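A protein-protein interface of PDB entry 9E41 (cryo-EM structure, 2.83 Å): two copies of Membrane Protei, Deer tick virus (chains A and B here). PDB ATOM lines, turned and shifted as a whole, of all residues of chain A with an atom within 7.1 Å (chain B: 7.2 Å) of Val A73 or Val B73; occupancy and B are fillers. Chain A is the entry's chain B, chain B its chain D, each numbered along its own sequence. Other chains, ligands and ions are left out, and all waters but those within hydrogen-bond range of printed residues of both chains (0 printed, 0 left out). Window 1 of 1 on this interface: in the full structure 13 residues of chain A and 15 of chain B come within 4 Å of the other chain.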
ATOM      1  N   THR A   6     -25.203 -19.074 -13.985  1.00  0.00           N
ATOM      2  CA  THR A   6     -25.731 -17.752 -14.287  1.00  0.00           C
ATOM      3  C   THR A   6     -26.475 -17.182 -13.085  1.00  0.00           C
ATOM      4  O   THR A   6     -27.134 -17.903 -12.329  1.00  0.00           O
ATOM      5  CB  THR A   6     -26.667 -17.810 -15.494  1.00  0.00           C
ATOM      6  OG1 THR A   6     -26.004 -18.457 -16.586  1.00  0.00           O
ATOM      7  CG2 THR A   6     -27.083 -16.405 -15.911  1.00  0.00           C
ATOM      8  N   HIS A  28     -28.598 -17.602 -26.512  1.00  0.00           N
ATOM      9  CA  HIS A  28     -29.345 -18.820 -26.817  1.00  0.00           C
ATOM     10  C   HIS A  28     -29.863 -18.795 -28.250  1.00  0.00           C
ATOM     11  O   HIS A  28     -29.779 -19.795 -28.976  1.00  0.00           O
ATOM     12  CB  HIS A  28     -30.502 -18.981 -25.832  1.00  0.00           C
ATOM     13  CG  HIS A  28     -30.067 -19.187 -24.414  1.00  0.00           C
ATOM     14  ND1 HIS A  28     -28.941 -19.906 -24.078  1.00  0.00           N
ATOM     15  CD2 HIS A  28     -30.606 -18.766 -23.245  1.00  0.00           C
ATOM     16  CE1 HIS A  28     -28.806 -19.921 -22.765  1.00  0.00           C
ATOM     17  NE2 HIS A  28     -29.802 -19.235 -22.235  1.00  0.00           N
ATOM     18  N   ARG A  31     -27.008 -19.319 -30.686  1.00  0.00           N
ATOM     19  CA  ARG A  31     -26.572 -20.710 -30.677  1.00  0.00           C
ATOM     20  C   ARG A  31     -27.533 -21.584 -31.471  1.00  0.00           C
ATOM     21  O   ARG A  31     -27.112 -22.395 -32.309  1.00  0.00           O
ATOM     22  CB  ARG A  31     -26.451 -21.192 -29.231  1.00  0.00           C
ATOM     23  CG  ARG A  31     -25.658 -22.471 -29.047  1.00  0.00           C
ATOM     24  CD  ARG A  31     -25.797 -22.997 -27.629  1.00  0.00           C
ATOM     25  NE  ARG A  31     -25.672 -21.924 -26.650  1.00  0.00           N
ATOM     26  CZ  ARG A  31     -24.520 -21.455 -26.189  1.00  0.00           C
ATOM     27  NH1 ARG A  31     -23.361 -21.966 -26.573  1.00  0.00           N
ATOM     28  NH2 ARG A  31     -24.530 -20.447 -25.322  1.00  0.00           N
ATOM     29  N   VAL A  32     -28.837 -21.417 -31.238  1.00  0.00           N
ATOM     30  CA  VAL A  32     -29.822 -22.233 -31.939  1.00  0.00           C
ATOM     31  C   VAL A  32     -29.791 -21.940 -33.434  1.00  0.00           C
ATOM     32  O   VAL A  32     -29.848 -22.859 -34.257  1.00  0.00           O
ATOM     33  CB  VAL A  32     -31.224 -22.007 -31.345  1.00  0.00           C
ATOM     34  CG1 VAL A  32     -32.291 -22.648 -32.222  1.00  0.00           C
ATOM     35  CG2 VAL A  32     -31.284 -22.557 -29.932  1.00  0.00           C
ATOM     36  N   TRP A  35     -26.649 -23.541 -34.992  1.00  0.00           N
ATOM     37  CA  TRP A  35     -26.762 -24.993 -35.078  1.00  0.00           C
ATOM     38  C   TRP A  35     -27.747 -25.400 -36.168  1.00  0.00           C
ATOM     39  O   TRP A  35     -27.506 -26.362 -36.903  1.00  0.00           O
ATOM     40  CB  TRP A  35     -27.178 -25.561 -33.723  1.00  0.00           C
ATOM     41  CG  TRP A  35     -27.199 -27.053 -33.676  1.00  0.00           C
ATOM     42  CD1 TRP A  35     -26.171 -27.874 -33.321  1.00  0.00           C
ATOM     43  CD2 TRP A  35     -28.305 -27.907 -33.987  1.00  0.00           C
ATOM     44  NE1 TRP A  35     -26.566 -29.187 -33.395  1.00  0.00           N
ATOM     45  CE2 TRP A  35     -27.873 -29.233 -33.801  1.00  0.00           C
ATOM     46  CE3 TRP A  35     -29.619 -27.678 -34.405  1.00  0.00           C
ATOM     47  CZ2 TRP A  35     -28.706 -30.327 -34.019  1.00  0.00           C
ATOM     48  CZ3 TRP A  35     -30.443 -28.763 -34.621  1.00  0.00           C
ATOM     49  CH2 TRP A  35     -29.986 -30.071 -34.428  1.00  0.00           C
ATOM     50  N   LEU A  68     -34.761 -28.861 -31.157  1.00  0.00           N
ATOM     51  CA  LEU A  68     -33.936 -27.712 -31.508  1.00  0.00           C
ATOM     52  C   LEU A  68     -33.256 -27.109 -30.287  1.00  0.00           C
ATOM     53  O   LEU A  68     -32.126 -26.617 -30.387  1.00  0.00           O
ATOM     54  CB  LEU A  68     -34.778 -26.650 -32.212  1.00  0.00           C
ATOM     55  CG  LEU A  68     -34.934 -26.819 -33.726  1.00  0.00           C
ATOM     56  CD1 LEU A  68     -35.816 -27.998 -34.100  1.00  0.00           C
ATOM     57  CD2 LEU A  68     -35.475 -25.531 -34.314  1.00  0.00           C
ATOM     58  N   SER A  69     -33.924 -27.125 -29.135  1.00  0.00           N
ATOM     59  CA  SER A  69     -33.355 -26.543 -27.928  1.00  0.00           C
ATOM     60  C   SER A  69     -32.301 -27.442 -27.292  1.00  0.00           C
ATOM     61  O   SER A  69     -31.319 -26.934 -26.738  1.00  0.00           O
ATOM     62  CB  SER A  69     -34.470 -26.249 -26.928  1.00  0.00           C
ATOM     63  OG  SER A  69     -35.068 -27.449 -26.476  1.00  0.00           O
ATOM     64  N   LEU A  70     -32.476 -28.762 -27.356  1.00  0.00           N
ATOM     65  CA  LEU A  70     -31.559 -29.684 -26.699  1.00  0.00           C
ATOM     66  C   LEU A  70     -30.395 -30.113 -27.582  1.00  0.00           C
ATOM     67  O   LEU A  70     -29.409 -30.645 -27.060  1.00  0.00           O
ATOM     68  CB  LEU A  70     -32.314 -30.935 -26.229  1.00  0.00           C
ATOM     69  CG  LEU A  70     -33.155 -30.856 -24.946  1.00  0.00           C
ATOM     70  CD1 LEU A  70     -33.664 -32.236 -24.542  1.00  0.00           C
ATOM     71  CD2 LEU A  70     -32.379 -30.234 -23.792  1.00  0.00           C
ATOM     72  N   GLY A  71     -30.474 -29.898 -28.895  1.00  0.00           N
ATOM     73  CA  GLY A  71     -29.390 -30.265 -29.775  1.00  0.00           C
ATOM     74  C   GLY A  71     -28.112 -29.496 -29.505  1.00  0.00           C
ATOM     75  O   GLY A  71     -27.111 -30.053 -29.043  1.00  0.00           O
ATOM     76  N   PRO A  72     -28.120 -28.191 -29.791  1.00  0.00           N
ATOM     77  CA  PRO A  72     -26.876 -27.414 -29.652  1.00  0.00           C
ATOM     78  C   PRO A  72     -26.303 -27.403 -28.249  1.00  0.00           C
ATOM     79  O   PRO A  72     -25.078 -27.437 -28.084  1.00  0.00           O
ATOM     80  CB  PRO A  72     -27.296 -26.006 -30.095  1.00  0.00           C
ATOM     81  CG  PRO A  72     -28.772 -25.963 -29.922  1.00  0.00           C
ATOM     82  CD  PRO A  72     -29.262 -27.350 -30.185  1.00  0.00           C
ATOM     83  N   VAL A  73     -27.155 -27.353 -27.227  1.00  0.00           N
ATOM     84  CA  VAL A  73     -26.663 -27.161 -25.868  1.00  0.00           C
ATOM     85  C   VAL A  73     -25.890 -28.385 -25.398  1.00  0.00           C
ATOM     86  O   VAL A  73     -24.796 -28.270 -24.835  1.00  0.00           O
ATOM     87  CB  VAL A  73     -27.826 -26.834 -24.919  1.00  0.00           C
ATOM     88  CG1 VAL A  73     -27.314 -26.750 -23.501  1.00  0.00           C
ATOM     89  CG2 VAL A  73     -28.503 -25.539 -25.347  1.00  0.00           C
ATOM     90  N   TYR A  74     -26.444 -29.576 -25.622  1.00  0.00           N
ATOM     91  CA  TYR A  74     -25.829 -30.820 -25.177  1.00  0.00           C
ATOM     92  C   TYR A  74     -24.960 -31.460 -26.251  1.00  0.00           C
ATOM     93  O   TYR A  74     -24.836 -32.690 -26.297  1.00  0.00           O
ATOM     94  CB  TYR A  74     -26.911 -31.792 -24.704  1.00  0.00           C
ATOM     95  CG  TYR A  74     -27.389 -31.510 -23.300  1.00  0.00           C
ATOM     96  CD1 TYR A  74     -28.410 -30.602 -23.058  1.00  0.00           C
ATOM     97  CD2 TYR A  74     -26.808 -32.144 -22.213  1.00  0.00           C
ATOM     98  CE1 TYR A  74     -28.843 -30.340 -21.774  1.00  0.00           C
ATOM     99  CE2 TYR A  74     -27.233 -31.888 -20.926  1.00  0.00           C
ATOM    100  CZ  TYR A  74     -28.251 -30.987 -20.714  1.00  0.00           C
ATOM    101  OH  TYR A  74     -28.676 -30.728 -19.431  1.00  0.00           O
ATOM    102  N   ALA A  75     -24.348 -30.654 -27.112  1.00  0.00           N
ATOM    103  CA  ALA A  75     -23.457 -31.169 -28.142  1.00  0.00           C
ATOM    104  C   ALA A  75     -22.171 -31.700 -27.519  1.00  0.00           C
ATOM    105  O   ALA A  75     -21.924 -31.532 -26.324  1.00  0.00           O
ATOM    106  CB  ALA A  75     -23.147 -30.089 -29.159  1.00  0.00           C
ATOM    107  OXT ALA A  75     -21.347 -32.314 -28.195  1.00  0.00           O
ATOM    108  N   THR B   6     -18.956 -25.786 -29.515  1.00  0.00           N
ATOM    109  CA  THR B   6     -17.981 -26.841 -29.282  1.00  0.00           C
ATOM    110  C   THR B   6     -17.600 -27.525 -30.590  1.00  0.00           C
ATOM    111  O   THR B   6     -18.392 -27.604 -31.534  1.00  0.00           O
ATOM    112  CB  THR B   6     -18.537 -27.871 -28.299  1.00  0.00           C
ATOM    113  OG1 THR B   6     -19.613 -28.589 -28.911  1.00  0.00           O
ATOM    114  CG2 THR B   6     -19.044 -27.182 -27.042  1.00  0.00           C
ATOM    115  N   HIS B  28     -21.670 -30.855 -18.056  1.00  0.00           N
ATOM    116  CA  HIS B  28     -23.126 -30.958 -18.084  1.00  0.00           C
ATOM    117  C   HIS B  28     -23.654 -31.636 -16.826  1.00  0.00           C
ATOM    118  O   HIS B  28     -24.644 -31.185 -16.233  1.00  0.00           O
ATOM    119  CB  HIS B  28     -23.572 -31.729 -19.326  1.00  0.00           C
ATOM    120  CG  HIS B  28     -23.324 -31.006 -20.614  1.00  0.00           C
ATOM    121  ND1 HIS B  28     -23.081 -31.662 -21.801  1.00  0.00           N
ATOM    122  CD2 HIS B  28     -23.286 -29.684 -20.901  1.00  0.00           C
ATOM    123  CE1 HIS B  28     -22.899 -30.776 -22.764  1.00  0.00           C
ATOM    124  NE2 HIS B  28     -23.018 -29.567 -22.244  1.00  0.00           N
ATOM    125  N   ARG B  31     -23.390 -29.280 -13.886  1.00  0.00           N
ATOM    126  CA  ARG B  31     -24.398 -28.229 -13.975  1.00  0.00           C
ATOM    127  C   ARG B  31     -25.763 -28.742 -13.537  1.00  0.00           C
ATOM    128  O   ARG B  31     -26.466 -28.087 -12.757  1.00  0.00           O
ATOM    129  CB  ARG B  31     -24.459 -27.694 -15.406  1.00  0.00           C
ATOM    130  CG  ARG B  31     -25.296 -26.438 -15.576  1.00  0.00           C
ATOM    131  CD  ARG B  31     -25.509 -26.124 -17.050  1.00  0.00           C
ATOM    132  NE  ARG B  31     -24.287 -26.273 -17.832  1.00  0.00           N
ATOM    133  CZ  ARG B  31     -23.306 -25.383 -17.878  1.00  0.00           C
ATOM    134  NH1 ARG B  31     -23.358 -24.256 -17.186  1.00  0.00           N
ATOM    135  NH2 ARG B  31     -22.242 -25.628 -18.639  1.00  0.00           N
ATOM    136  N   VAL B  32     -26.156 -29.919 -14.029  1.00  0.00           N
ATOM    137  CA  VAL B  32     -27.457 -30.468 -13.652  1.00  0.00           C
ATOM    138  C   VAL B  32     -27.512 -30.727 -12.153  1.00  0.00           C
ATOM    139  O   VAL B  32     -28.508 -30.408 -11.490  1.00  0.00           O
ATOM    140  CB  VAL B  32     -27.762 -31.742 -14.461  1.00  0.00           C
ATOM    141  CG1 VAL B  32     -29.021 -32.414 -13.935  1.00  0.00           C
ATOM    142  CG2 VAL B  32     -27.926 -31.402 -15.931  1.00  0.00           C
ATOM    143  N   TRP B  35     -27.816 -27.417 -10.238  1.00  0.00           N
ATOM    144  CA  TRP B  35     -29.162 -26.869 -10.353  1.00  0.00           C
ATOM    145  C   TRP B  35     -30.141 -27.636  -9.475  1.00  0.00           C
ATOM    146  O   TRP B  35     -30.991 -27.037  -8.807  1.00  0.00           O
ATOM    147  CB  TRP B  35     -29.621 -26.904 -11.808  1.00  0.00           C
ATOM    148  CG  TRP B  35     -30.964 -26.276 -12.023  1.00  0.00           C
ATOM    149  CD1 TRP B  35     -31.220 -24.960 -12.276  1.00  0.00           C
ATOM    150  CD2 TRP B  35     -32.238 -26.931 -11.978  1.00  0.00           C
ATOM    151  NE1 TRP B  35     -32.572 -24.758 -12.407  1.00  0.00           N
ATOM    152  CE2 TRP B  35     -33.219 -25.952 -12.227  1.00  0.00           C
ATOM    153  CE3 TRP B  35     -32.643 -28.251 -11.757  1.00  0.00           C
ATOM    154  CZ2 TRP B  35     -34.579 -26.250 -12.260  1.00  0.00           C
ATOM    155  CZ3 TRP B  35     -33.991 -28.544 -11.793  1.00  0.00           C
ATOM    156  CH2 TRP B  35     -34.944 -27.548 -12.042  1.00  0.00           C
ATOM    157  N   LEU B  68     -35.216 -31.642 -16.167  1.00  0.00           N
ATOM    158  CA  LEU B  68     -33.964 -31.427 -15.448  1.00  0.00           C
ATOM    159  C   LEU B  68     -32.837 -31.009 -16.381  1.00  0.00           C
ATOM    160  O   LEU B  68     -32.006 -30.176 -16.006  1.00  0.00           O
ATOM    161  CB  LEU B  68     -33.565 -32.683 -14.673  1.00  0.00           C
ATOM    162  CG  LEU B  68     -34.535 -33.185 -13.601  1.00  0.00           C
ATOM    163  CD1 LEU B  68     -33.830 -34.185 -12.696  1.00  0.00           C
ATOM    164  CD2 LEU B  68     -35.130 -32.044 -12.780  1.00  0.00           C
ATOM    165  N   SER B  69     -32.776 -31.578 -17.582  1.00  0.00           N
ATOM    166  CA  SER B  69     -31.717 -31.244 -18.525  1.00  0.00           C
ATOM    167  C   SER B  69     -31.974 -29.951 -19.283  1.00  0.00           C
ATOM    168  O   SER B  69     -31.026 -29.370 -19.824  1.00  0.00           O
ATOM    169  CB  SER B  69     -31.534 -32.386 -19.528  1.00  0.00           C
ATOM    170  OG  SER B  69     -32.446 -32.266 -20.605  1.00  0.00           O
ATOM    171  N   LEU B  70     -33.219 -29.478 -19.329  1.00  0.00           N
ATOM    172  CA  LEU B  70     -33.569 -28.281 -20.078  1.00  0.00           C
ATOM    173  C   LEU B  70     -33.691 -27.042 -19.202  1.00  0.00           C
ATOM    174  O   LEU B  70     -33.660 -25.927 -19.731  1.00  0.00           O
ATOM    175  CB  LEU B  70     -34.890 -28.513 -20.824  1.00  0.00           C
ATOM    176  CG  LEU B  70     -35.384 -27.435 -21.792  1.00  0.00           C
ATOM    177  CD1 LEU B  70     -34.418 -27.253 -22.949  1.00  0.00           C
ATOM    178  CD2 LEU B  70     -36.766 -27.792 -22.308  1.00  0.00           C
ATOM    179  N   GLY B  71     -33.827 -27.202 -17.888  1.00  0.00           N
ATOM    180  CA  GLY B  71     -33.889 -26.070 -16.998  1.00  0.00           C
ATOM    181  C   GLY B  71     -32.575 -25.321 -16.877  1.00  0.00           C
ATOM    182  O   GLY B  71     -32.453 -24.170 -17.309  1.00  0.00           O
ATOM    183  N   PRO B  72     -31.558 -25.966 -16.296  1.00  0.00           N
ATOM    184  CA  PRO B  72     -30.337 -25.223 -15.930  1.00  0.00           C
ATOM    185  C   PRO B  72     -29.659 -24.507 -17.082  1.00  0.00           C
ATOM    186  O   PRO B  72     -29.159 -23.390 -16.896  1.00  0.00           O
ATOM    187  CB  PRO B  72     -29.430 -26.317 -15.349  1.00  0.00           C
ATOM    188  CG  PRO B  72     -29.988 -27.607 -15.833  1.00  0.00           C
ATOM    189  CD  PRO B  72     -31.458 -27.394 -15.961  1.00  0.00           C
ATOM    190  N   VAL B  73     -29.607 -25.117 -18.265  1.00  0.00           N
ATOM    191  CA  VAL B  73     -28.833 -24.530 -19.354  1.00  0.00           C
ATOM    192  C   VAL B  73     -29.503 -23.267 -19.877  1.00  0.00           C
ATOM    193  O   VAL B  73     -28.828 -22.305 -20.260  1.00  0.00           O
ATOM    194  CB  VAL B  73     -28.609 -25.565 -20.470  1.00  0.00           C
ATOM    195  CG1 VAL B  73     -27.905 -26.799 -19.918  1.00  0.00           C
ATOM    196  CG2 VAL B  73     -29.927 -25.939 -21.123  1.00  0.00           C
ATOM    197  N   TYR B  74     -30.834 -23.245 -19.912  1.00  0.00           N
ATOM    198  CA  TYR B  74     -31.578 -22.083 -20.380  1.00  0.00           C
ATOM    199  C   TYR B  74     -31.894 -21.100 -19.260  1.00  0.00           C
ATOM    200  O   TYR B  74     -32.884 -20.368 -19.353  1.00  0.00           O
ATOM    201  CB  TYR B  74     -32.870 -22.529 -21.073  1.00  0.00           C
ATOM    202  CG  TYR B  74     -32.650 -23.035 -22.480  1.00  0.00           C
ATOM    203  CD1 TYR B  74     -32.592 -22.159 -23.557  1.00  0.00           C
ATOM    204  CD2 TYR B  74     -32.509 -24.390 -22.734  1.00  0.00           C
ATOM    205  CE1 TYR B  74     -32.390 -22.622 -24.843  1.00  0.00           C
ATOM    206  CE2 TYR B  74     -32.306 -24.859 -24.014  1.00  0.00           C
ATOM    207  CZ  TYR B  74     -32.248 -23.973 -25.064  1.00  0.00           C
ATOM    208  OH  TYR B  74     -32.047 -24.445 -26.340  1.00  0.00           O
ATOM    209  N   ALA B  75     -31.077 -21.066 -18.212  1.00  0.00           N
ATOM    210  CA  ALA B  75     -31.257 -20.115 -17.124  1.00  0.00           C
ATOM    211  C   ALA B  75     -30.450 -18.846 -17.386  1.00  0.00           C
ATOM    212  O   ALA B  75     -29.736 -18.746 -18.384  1.00  0.00           O
ATOM    213  CB  ALA B  75     -30.849 -20.739 -15.804  1.00  0.00           C
ATOM    214  OXT ALA B  75     -30.494 -17.893 -16.610  1.00  0.00           O
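His A28 touches Val B73, and with the chains exchanged Val A73 touches His B28. His A28 touches Ala B75, and with the chains exchanged Ala A75 touches His B28. Ser A69 touches Tyr B74, and with the chains exchanged Tyr A74 touches Ser B69. Val A73 touches Tyr B74, but with the chains exchanged Tyr A74 does not touch Val B73 (4.03 Å). 13 positions are printed for both chains. Of the 16 pairs that touch across the chains among the printed residues, 14 have their exchanged pair printed and touching as well.
O of Val B73 touches CE1 of His A28, at 3.5 Å. Tyr B74 touches His A28 (CA to NE2, 3.8 Å). NE2 of His A28 touches O of Ala B75 (3.9 Å). OG of Ser A69 touches CD1 of Leu B70 (3.6 Å). CG1 of Val A73 touches CB of Val B73, 3.5 Å away. CG2 of Val A73 touches OH of Tyr B74 (3.8 Å). Tyr A74 touches His B28. Tyr A74 touches Val B32. OG1 of Thr B6 touches CB of Ala A75 (3.8 Å). CE1 of His B28 touches O of Ala A75 (3.8 Å).
Of chain B, only His B28, Val B73 and Tyr B74 come within 4 Å of Val A73. Val B73 touches just these residues of chain A: His A28 and Val A73. Printed residues of chain B within 4 Å of Tyr A74: His B28 (3.8 Å), Val B32 (3.6 Å) and Ser B69 (2.7 Å). Of the printed residues of chain A, Thr B6 touches Ala A75. Pro B72 touches none of the printed residues of chain A. The nearest printed residue of chain B that does not touch Leu A70 is Tyr B74 (4.5 Å).
O of Ser A69 is in hydrogen-bond range of OH of Tyr B74. The backbone carbonyl oxygen (O) of Val A73 is in hydrogen-bond range of a ring nitrogen (NE2) of His B28, at 3.4 Å. The backbone carbonyl oxygen (O) of Ser B69 sits at hydrogen-bond distance from the side-chain hydroxyl (OH) of Tyr A74, 2.7 Å away.
Printed residues of chain B that touch a printed residue of chain A: Thr B6, His B28, Val B32, Ser B69, Leu B70, Val B73, Tyr B74 and Ala B75. Of the 13 printed residues of chain A, 7 touch a printed residue of chain B. Hydrophobic or aromatic side chains of chain A within 4 Å of the printed part of chain B: His A28, Leu A70, Val A73, Tyr A74 and Ala A75. Among the printed residues, no Asp or Glu carboxylate lies within 4 Å of a Lys or Arg side-chain nitrogen of the other chain.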
